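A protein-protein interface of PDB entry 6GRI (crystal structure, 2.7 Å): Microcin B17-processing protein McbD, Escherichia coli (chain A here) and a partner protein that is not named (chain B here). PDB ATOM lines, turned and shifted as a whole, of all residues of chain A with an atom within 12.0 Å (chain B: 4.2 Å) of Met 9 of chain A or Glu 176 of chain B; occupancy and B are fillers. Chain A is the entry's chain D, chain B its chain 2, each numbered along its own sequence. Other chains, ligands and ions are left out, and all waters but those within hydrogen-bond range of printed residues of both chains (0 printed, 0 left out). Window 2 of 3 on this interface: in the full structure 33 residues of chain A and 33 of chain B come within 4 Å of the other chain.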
ATOM      1  N   TYR A   5     -29.379  31.368   9.962  1.00  0.00           N
ATOM      2  CA  TYR A   5     -28.165  31.393  10.747  1.00  0.00           C
ATOM      3  C   TYR A   5     -27.899  29.979  11.228  1.00  0.00           C
ATOM      4  O   TYR A   5     -28.838  29.228  11.503  1.00  0.00           O
ATOM      5  CB  TYR A   5     -28.323  32.339  11.935  1.00  0.00           C
ATOM      6  CG  TYR A   5     -28.805  33.726  11.555  1.00  0.00           C
ATOM      7  CD1 TYR A   5     -28.105  34.509  10.624  1.00  0.00           C
ATOM      8  CD2 TYR A   5     -29.972  34.256  12.110  1.00  0.00           C
ATOM      9  CE1 TYR A   5     -28.557  35.787  10.271  1.00  0.00           C
ATOM     10  CE2 TYR A   5     -30.429  35.526  11.774  1.00  0.00           C
ATOM     11  CZ  TYR A   5     -29.726  36.294  10.865  1.00  0.00           C
ATOM     12  OH  TYR A   5     -30.201  37.550  10.551  1.00  0.00           O
ATOM     13  N   SER A   6     -26.623  29.614  11.306  1.00  0.00           N
ATOM     14  CA  SER A   6     -26.194  28.325  11.874  1.00  0.00           C
ATOM     15  C   SER A   6     -25.071  28.551  12.897  1.00  0.00           C
ATOM     16  O   SER A   6     -24.187  29.392  12.681  1.00  0.00           O
ATOM     17  CB  SER A   6     -25.715  27.386  10.757  1.00  0.00           C
ATOM     18  OG  SER A   6     -26.670  27.283   9.714  1.00  0.00           O
ATOM     19  N   ASN A   7     -25.090  27.799  13.995  1.00  0.00           N
ATOM     20  CA  ASN A   7     -24.061  27.940  15.038  1.00  0.00           C
ATOM     21  C   ASN A   7     -22.677  27.394  14.598  1.00  0.00           C
ATOM     22  O   ASN A   7     -22.515  26.884  13.476  1.00  0.00           O
ATOM     23  CB  ASN A   7     -24.541  27.346  16.385  1.00  0.00           C
ATOM     24  CG  ASN A   7     -24.643  25.825  16.387  1.00  0.00           C
ATOM     25  OD1 ASN A   7     -23.806  25.114  15.814  1.00  0.00           O
ATOM     26  ND2 ASN A   7     -25.660  25.315  17.077  1.00  0.00           N
ATOM     27  N   LEU A   8     -21.688  27.529  15.485  1.00  0.00           N
ATOM     28  CA  LEU A   8     -20.317  27.075  15.226  1.00  0.00           C
ATOM     29  C   LEU A   8     -20.194  25.541  15.092  1.00  0.00           C
ATOM     30  O   LEU A   8     -19.269  25.054  14.430  1.00  0.00           O
ATOM     31  CB  LEU A   8     -19.362  27.603  16.310  1.00  0.00           C
ATOM     32  N   MET A   9     -21.132  24.796  15.692  1.00  0.00           N
ATOM     33  CA  MET A   9     -21.175  23.319  15.582  1.00  0.00           C
ATOM     34  C   MET A   9     -21.903  22.749  14.332  1.00  0.00           C
ATOM     35  O   MET A   9     -22.039  21.527  14.201  1.00  0.00           O
ATOM     36  CB  MET A   9     -21.744  22.730  16.873  1.00  0.00           C
ATOM     37  CG  MET A   9     -20.798  22.905  18.053  1.00  0.00           C
ATOM     38  SD  MET A   9     -21.565  23.589  19.531  1.00  0.00           S
ATOM     39  CE  MET A   9     -21.602  25.335  19.114  1.00  0.00           C
ATOM     40  N   SER A  10     -22.316  23.616  13.402  1.00  0.00           N
ATOM     41  CA  SER A  10     -23.134  23.207  12.261  1.00  0.00           C
ATOM     42  C   SER A  10     -22.294  22.792  11.075  1.00  0.00           C
ATOM     43  O   SER A  10     -21.129  23.168  10.966  1.00  0.00           O
ATOM     44  CB  SER A  10     -24.049  24.350  11.838  1.00  0.00           C
ATOM     45  OG  SER A  10     -24.878  23.962  10.761  1.00  0.00           O
ATOM     46  N   ALA A  11     -22.906  22.018  10.184  1.00  0.00           N
ATOM     47  CA  ALA A  11     -22.339  21.740   8.859  1.00  0.00           C
ATOM     48  C   ALA A  11     -22.595  22.892   7.884  1.00  0.00           C
ATOM     49  O   ALA A  11     -21.989  22.952   6.804  1.00  0.00           O
ATOM     50  CB  ALA A  11     -22.931  20.459   8.295  1.00  0.00           C
ATOM     51  N   TRP A  12     -23.493  23.798   8.270  1.00  0.00           N
ATOM     52  CA  TRP A  12     -24.019  24.821   7.388  1.00  0.00           C
ATOM     53  C   TRP A  12     -23.430  26.177   7.733  1.00  0.00           C
ATOM     54  O   TRP A  12     -23.122  26.439   8.907  1.00  0.00           O
ATOM     55  CB  TRP A  12     -25.544  24.825   7.501  1.00  0.00           C
ATOM     56  CG  TRP A  12     -26.090  23.499   7.098  1.00  0.00           C
ATOM     57  CD1 TRP A  12     -26.506  22.494   7.921  1.00  0.00           C
ATOM     58  CD2 TRP A  12     -26.206  23.004   5.763  1.00  0.00           C
ATOM     59  NE1 TRP A  12     -26.902  21.413   7.180  1.00  0.00           N
ATOM     60  CE2 TRP A  12     -26.728  21.698   5.849  1.00  0.00           C
ATOM     61  CE3 TRP A  12     -25.939  23.548   4.501  1.00  0.00           C
ATOM     62  CZ2 TRP A  12     -26.986  20.917   4.715  1.00  0.00           C
ATOM     63  CZ3 TRP A  12     -26.191  22.769   3.369  1.00  0.00           C
ATOM     64  CH2 TRP A  12     -26.711  21.467   3.490  1.00  0.00           C
ATOM     65  N   PRO A  13     -23.275  27.048   6.714  1.00  0.00           N
ATOM     66  CA  PRO A  13     -22.624  28.335   6.944  1.00  0.00           C
ATOM     67  C   PRO A  13     -23.367  29.215   7.949  1.00  0.00           C
ATOM     68  O   PRO A  13     -24.565  29.037   8.177  1.00  0.00           O
ATOM     69  CB  PRO A  13     -22.633  28.981   5.567  1.00  0.00           C
ATOM     70  CG  PRO A  13     -23.794  28.371   4.882  1.00  0.00           C
ATOM     71  CD  PRO A  13     -23.833  26.958   5.352  1.00  0.00           C
ATOM     72  N   ALA A  14     -22.638  30.163   8.519  1.00  0.00           N
ATOM     73  CA  ALA A  14     -23.153  31.040   9.547  1.00  0.00           C
ATOM     74  C   ALA A  14     -24.317  31.924   9.086  1.00  0.00           C
ATOM     75  O   ALA A  14     -25.179  32.242   9.896  1.00  0.00           O
ATOM     76  CB  ALA A  14     -22.026  31.906  10.096  1.00  0.00           C
ATOM     77  N   THR A  15     -24.333  32.336   7.815  1.00  0.00           N
ATOM     78  CA  THR A  15     -25.370  33.254   7.299  1.00  0.00           C
ATOM     79  C   THR A  15     -25.676  33.002   5.826  1.00  0.00           C
ATOM     80  O   THR A  15     -24.764  32.777   5.036  1.00  0.00           O
ATOM     81  CB  THR A  15     -24.959  34.754   7.438  1.00  0.00           C
ATOM     82  OG1 THR A  15     -24.786  35.101   8.818  1.00  0.00           O
ATOM     83  CG2 THR A  15     -26.020  35.693   6.854  1.00  0.00           C
ATOM     84  N   ASP A  34     -19.424  32.762   5.579  1.00  0.00           N
ATOM     85  CA  ASP A  34     -18.878  31.862   6.608  1.00  0.00           C
ATOM     86  C   ASP A  34     -17.337  31.817   6.663  1.00  0.00           C
ATOM     87  O   ASP A  34     -16.714  30.877   6.153  1.00  0.00           O
ATOM     88  CB  ASP A  34     -19.429  30.434   6.430  1.00  0.00           C
ATOM     89  CG  ASP A  34     -19.150  29.549   7.632  1.00  0.00           C
ATOM     90  OD1 ASP A  34     -19.494  29.955   8.765  1.00  0.00           O
ATOM     91  OD2 ASP A  34     -18.596  28.443   7.449  1.00  0.00           O
ATOM     92  N   TYR A  35     -16.731  32.832   7.278  1.00  0.00           N
ATOM     93  CA  TYR A  35     -15.296  32.798   7.650  1.00  0.00           C
ATOM     94  C   TYR A  35     -14.299  32.525   6.502  1.00  0.00           C
ATOM     95  O   TYR A  35     -13.803  31.412   6.316  1.00  0.00           O
ATOM     96  CB  TYR A  35     -15.103  31.807   8.808  1.00  0.00           C
ATOM     97  CG  TYR A  35     -16.100  32.056   9.926  1.00  0.00           C
ATOM     98  CD1 TYR A  35     -16.120  33.280  10.604  1.00  0.00           C
ATOM     99  CD2 TYR A  35     -17.048  31.092  10.281  1.00  0.00           C
ATOM    100  CE1 TYR A  35     -17.042  33.530  11.610  1.00  0.00           C
ATOM    101  CE2 TYR A  35     -17.978  31.338  11.288  1.00  0.00           C
ATOM    102  CZ  TYR A  35     -17.970  32.558  11.949  1.00  0.00           C
ATOM    103  OH  TYR A  35     -18.879  32.815  12.953  1.00  0.00           O
ATOM    104  N   TYR A  58     -21.799  28.797  -3.281  1.00  0.00           N
ATOM    105  CA  TYR A  58     -21.248  28.309  -2.015  1.00  0.00           C
ATOM    106  C   TYR A  58     -20.911  26.813  -2.088  1.00  0.00           C
ATOM    107  O   TYR A  58     -19.836  26.394  -1.646  1.00  0.00           O
ATOM    108  CB  TYR A  58     -22.217  28.590  -0.842  1.00  0.00           C
ATOM    109  CG  TYR A  58     -21.772  27.976   0.472  1.00  0.00           C
ATOM    110  CD1 TYR A  58     -20.725  28.536   1.206  1.00  0.00           C
ATOM    111  CD2 TYR A  58     -22.376  26.818   0.972  1.00  0.00           C
ATOM    112  CE1 TYR A  58     -20.302  27.973   2.406  1.00  0.00           C
ATOM    113  CE2 TYR A  58     -21.956  26.248   2.174  1.00  0.00           C
ATOM    114  CZ  TYR A  58     -20.921  26.830   2.888  1.00  0.00           C
ATOM    115  OH  TYR A  58     -20.488  26.275   4.076  1.00  0.00           O
ATOM    116  N   ARG A  62     -17.075  25.167  -1.906  1.00  0.00           N
ATOM    117  CA  ARG A  62     -16.845  24.156  -0.882  1.00  0.00           C
ATOM    118  C   ARG A  62     -16.224  22.890  -1.463  1.00  0.00           C
ATOM    119  O   ARG A  62     -15.263  22.357  -0.909  1.00  0.00           O
ATOM    120  CB  ARG A  62     -18.155  23.798  -0.186  1.00  0.00           C
ATOM    121  CG  ARG A  62     -18.404  24.532   1.117  1.00  0.00           C
ATOM    122  CD  ARG A  62     -19.216  23.658   2.055  1.00  0.00           C
ATOM    123  NE  ARG A  62     -20.105  22.767   1.319  1.00  0.00           N
ATOM    124  CZ  ARG A  62     -21.088  22.063   1.869  1.00  0.00           C
ATOM    125  NH1 ARG A  62     -21.332  22.139   3.176  1.00  0.00           N
ATOM    126  NH2 ARG A  62     -21.829  21.281   1.103  1.00  0.00           N
ATOM    127  N   LEU B 174     -21.316  18.648  22.745  1.00  0.00           N
ATOM    128  CA  LEU B 174     -20.329  19.620  22.312  1.00  0.00           C
ATOM    129  C   LEU B 174     -20.550  20.897  23.109  1.00  0.00           C
ATOM    130  O   LEU B 174     -21.422  21.709  22.778  1.00  0.00           O
ATOM    131  CB  LEU B 174     -20.451  19.874  20.805  1.00  0.00           C
ATOM    132  CG  LEU B 174     -20.287  18.643  19.907  1.00  0.00           C
ATOM    133  CD1 LEU B 174     -20.385  19.064  18.452  1.00  0.00           C
ATOM    134  CD2 LEU B 174     -18.977  17.911  20.172  1.00  0.00           C
ATOM    135  N   LYS B 175     -19.766  21.037  24.180  1.00  0.00           N
ATOM    136  CA  LYS B 175     -19.853  22.157  25.123  1.00  0.00           C
ATOM    137  C   LYS B 175     -21.304  22.395  25.602  1.00  0.00           C
ATOM    138  O   LYS B 175     -21.789  21.633  26.439  1.00  0.00           O
ATOM    139  CB  LYS B 175     -19.189  23.408  24.532  1.00  0.00           C
ATOM    140  N   GLU B 176     -22.000  23.398  25.061  1.00  0.00           N
ATOM    141  CA  GLU B 176     -23.369  23.720  25.501  1.00  0.00           C
ATOM    142  C   GLU B 176     -24.469  22.973  24.714  1.00  0.00           C
ATOM    143  O   GLU B 176     -25.640  23.026  25.094  1.00  0.00           O
ATOM    144  CB  GLU B 176     -23.601  25.252  25.509  1.00  0.00           C
ATOM    145  CG  GLU B 176     -24.330  25.891  24.325  1.00  0.00           C
ATOM    146  CD  GLU B 176     -23.571  25.863  22.998  1.00  0.00           C
ATOM    147  OE1 GLU B 176     -22.344  25.597  22.965  1.00  0.00           O
ATOM    148  OE2 GLU B 176     -24.226  26.132  21.964  1.00  0.00           O
ATOM    149  N   SER B 177     -24.090  22.270  23.645  1.00  0.00           N
ATOM    150  CA  SER B 177     -25.052  21.654  22.740  1.00  0.00           C
ATOM    151  C   SER B 177     -25.094  20.145  22.871  1.00  0.00           C
ATOM    152  O   SER B 177     -24.054  19.503  22.866  1.00  0.00           O
ATOM    153  CB  SER B 177     -24.690  21.989  21.311  1.00  0.00           C
ATOM    154  OG  SER B 177     -25.635  21.409  20.438  1.00  0.00           O
ATOM    155  N   PHE B 178     -26.306  19.597  22.963  1.00  0.00           N
ATOM    156  CA  PHE B 178     -26.547  18.156  22.929  1.00  0.00           C
ATOM    157  C   PHE B 178     -26.920  17.768  21.501  1.00  0.00           C
ATOM    158  O   PHE B 178     -27.899  18.280  20.946  1.00  0.00           O
ATOM    159  CB  PHE B 178     -27.664  17.776  23.903  1.00  0.00           C
ATOM    160  CG  PHE B 178     -28.021  16.311  23.898  1.00  0.00           C
ATOM    161  CD1 PHE B 178     -27.043  15.333  24.032  1.00  0.00           C
ATOM    162  CD2 PHE B 178     -29.345  15.909  23.781  1.00  0.00           C
ATOM    163  CE1 PHE B 178     -27.379  13.987  24.041  1.00  0.00           C
ATOM    164  CE2 PHE B 178     -29.686  14.561  23.788  1.00  0.00           C
ATOM    165  CZ  PHE B 178     -28.702  13.599  23.917  1.00  0.00           C
ATOM    166  N   ARG B 179     -26.144  16.845  20.933  1.00  0.00           N
ATOM    167  CA  ARG B 179     -26.163  16.535  19.503  1.00  0.00           C
ATOM    168  C   ARG B 179     -26.792  15.176  19.250  1.00  0.00           C
ATOM    169  O   ARG B 179     -26.448  14.218  19.914  1.00  0.00           O
ATOM    170  CB  ARG B 179     -24.734  16.490  18.959  1.00  0.00           C
ATOM    171  CG  ARG B 179     -23.796  17.590  19.445  1.00  0.00           C
ATOM    172  CD  ARG B 179     -24.236  18.961  18.994  1.00  0.00           C
ATOM    173  NE  ARG B 179     -24.223  19.086  17.537  1.00  0.00           N
ATOM    174  CZ  ARG B 179     -24.578  20.184  16.879  1.00  0.00           C
ATOM    175  NH1 ARG B 179     -24.966  21.277  17.538  1.00  0.00           N
ATOM    176  NH2 ARG B 179     -24.550  20.189  15.550  1.00  0.00           N
ATOM    177  N   TRP B 200     -18.759  19.539   9.569  1.00  0.00           N
ATOM    178  CA  TRP B 200     -18.621  20.527  10.632  1.00  0.00           C
ATOM    179  C   TRP B 200     -17.250  21.155  10.584  1.00  0.00           C
ATOM    180  O   TRP B 200     -17.121  22.376  10.539  1.00  0.00           O
ATOM    181  CB  TRP B 200     -18.845  19.856  11.988  1.00  0.00           C
ATOM    182  CG  TRP B 200     -18.475  20.662  13.205  1.00  0.00           C
ATOM    183  CD1 TRP B 200     -18.587  22.018  13.381  1.00  0.00           C
ATOM    184  CD2 TRP B 200     -17.974  20.138  14.435  1.00  0.00           C
ATOM    185  NE1 TRP B 200     -18.157  22.366  14.643  1.00  0.00           N
ATOM    186  CE2 TRP B 200     -17.783  21.230  15.309  1.00  0.00           C
ATOM    187  CE3 TRP B 200     -17.659  18.848  14.881  1.00  0.00           C
ATOM    188  CZ2 TRP B 200     -17.291  21.074  16.599  1.00  0.00           C
ATOM    189  CZ3 TRP B 200     -17.165  18.691  16.173  1.00  0.00           C
ATOM    190  CH2 TRP B 200     -16.984  19.802  17.017  1.00  0.00           C
ATOM    191  N   ALA B 272     -29.537  20.440  20.333  1.00  0.00           N
ATOM    192  CA  ALA B 272     -30.285  20.997  21.464  1.00  0.00           C
ATOM    193  C   ALA B 272     -29.388  21.784  22.412  1.00  0.00           C
ATOM    194  O   ALA B 272     -28.606  21.201  23.161  1.00  0.00           O
ATOM    195  CB  ALA B 272     -31.008  19.889  22.217  1.00  0.00           C
ATOM    196  N   ASP B 273     -29.519  23.107  22.367  1.00  0.00           N
ATOM    197  CA  ASP B 273     -28.826  24.027  23.270  1.00  0.00           C
ATOM    198  C   ASP B 273     -29.355  23.764  24.681  1.00  0.00           C
ATOM    199  O   ASP B 273     -30.537  23.931  24.943  1.00  0.00           O
ATOM    200  CB  ASP B 273     -29.115  25.473  22.819  1.00  0.00           C
ATOM    201  CG  ASP B 273     -28.285  26.528  23.552  1.00  0.00           C
ATOM    202  OD1 ASP B 273     -28.256  26.512  24.797  1.00  0.00           O
ATOM    203  OD2 ASP B 273     -27.706  27.412  22.873  1.00  0.00           O
ATOM    204  N   LEU B 274     -28.474  23.335  25.577  1.00  0.00           N
ATOM    205  CA  LEU B 274     -28.841  22.998  26.949  1.00  0.00           C
ATOM    206  C   LEU B 274     -29.102  24.203  27.845  1.00  0.00           C
ATOM    207  O   LEU B 274     -29.724  24.059  28.902  1.00  0.00           O
ATOM    208  CB  LEU B 274     -27.753  22.144  27.589  1.00  0.00           C
ATOM    209  CG  LEU B 274     -27.485  20.800  26.932  1.00  0.00           C
ATOM    210  CD1 LEU B 274     -26.469  20.045  27.776  1.00  0.00           C
ATOM    211  CD2 LEU B 274     -28.760  19.977  26.772  1.00  0.00           C
ATOM    212  N   ILE B 275     -28.635  25.378  27.440  1.00  0.00           N
ATOM    213  CA  ILE B 275     -28.888  26.586  28.205  1.00  0.00           C
ATOM    214  C   ILE B 275     -30.309  27.075  27.904  1.00  0.00           C
ATOM    215  O   ILE B 275     -31.164  27.094  28.789  1.00  0.00           O
ATOM    216  CB  ILE B 275     -27.863  27.690  27.892  1.00  0.00           C
ATOM    217  CG1 ILE B 275     -26.426  27.189  28.109  1.00  0.00           C
ATOM    218  CG2 ILE B 275     -28.125  28.915  28.757  1.00  0.00           C
ATOM    219  CD1 ILE B 275     -25.411  27.930  27.256  1.00  0.00           C
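Tyr 5 of chain A touches none of the printed residues of chain B.
Asn 7 of chain A touches none of the printed residues of chain B.
Printed residues of chain B within 4 Å of Leu 8 of chain A: Trp 200 (2.9 Å).
Met 9 of chain A touches just these residues of chain B: Leu 174 (3.8 Å), Glu 176 (3.9 Å), Ser 177 (3.9 Å), Arg 179 (3.1 Å) and Trp 200 (3.3 Å).
No residue of chain A comes within 4 Å of Lys 175 of chain B.
Glu 176 of chain B touches one residue of chain A.
Ser 177 of chain B touches just one residue of chain A: Met 9 (3.9 Å).
Printed residues of chain A within 4 Å of Arg 179 of chain B: Met 9.
Trp 200 of chain B touches just these residues of chain A: Leu 8, Met 9 and Ser 10.
No residue of chain A comes within 4 Å of Ala 272 of chain B.
No residue of chain A comes within 4 Å of Asp 273 of chain B.
No residue of chain A comes within 4 Å of Leu 274 of chain B.
No residue of chain A comes within 4 Å of Ile 275 of chain B.
The nearest printed residue of chain B that does not touch Met 9 of chain A is Lys 175 of chain B (5.5 Å).
The nearest residue of chain A that does not touch Glu 176 of chain B is Asn 7 of chain A (5.2 Å).
Of the 11 printed residues of chain B, 5 touch a printed residue of chain A.
Hydrophobic or aromatic side chains of chain A within 4 Å of the printed part of chain B: Met 9.
Among the printed residues, 7 pairs touch across the chains.
Among the printed residues, no Asp or Glu carboxylate lies within 4 Å of a Lys or Arg side-chain nitrogen of the other chain.
NH1 of Arg 179 of chain B sits at hydrogen-bond distance from OG of Ser 177 of chain B, 3.0 Å away.
The backbone NH of Trp 12 of chain A is in hydrogen-bond range of the side-chain hydroxyl of Ser 10 of chain A (2.9 Å).
N of Leu 274 of chain B sits at hydrogen-bond distance from O of Glu 176 of chain B.
The side-chain amide oxygen (OD1) of Asn 7 of chain A is in hydrogen-bond range of the backbone NH (N) of Ser 10 of chain A (3.2 Å).
The side-chain amide oxygen of Asn 7 of chain A is in hydrogen-bond range of the backbone NH of Met 9 of chain A.
NH2 of Arg 179 of chain B is in hydrogen-bond range of O of Met 9 of chain A, 3.1 Å away.
The side-chain sulfur (SD) of Met 9 of chain A lies close to the backbone carbonyl oxygen (O) of Leu 174 of chain B.
The indole nitrogen (NE1) of Trp 200 of chain B is in hydrogen-bond range of the backbone carbonyl oxygen (O) of Leu 8 of chain A, at 2.9 Å.
OE1 of Glu 176 of chain B touches CE of Met 9 of chain A, at 3.9 Å.
Met 9 of chain A touches Ser 177 of chain B (SD to CB, 3.9 Å).
NE1 of Trp 200 of chain B touches CA of Met 9 of chain A (3.3 Å).
Ser 10 of chain A touches Trp 200 of chain B (O to CA, 3.7 Å).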
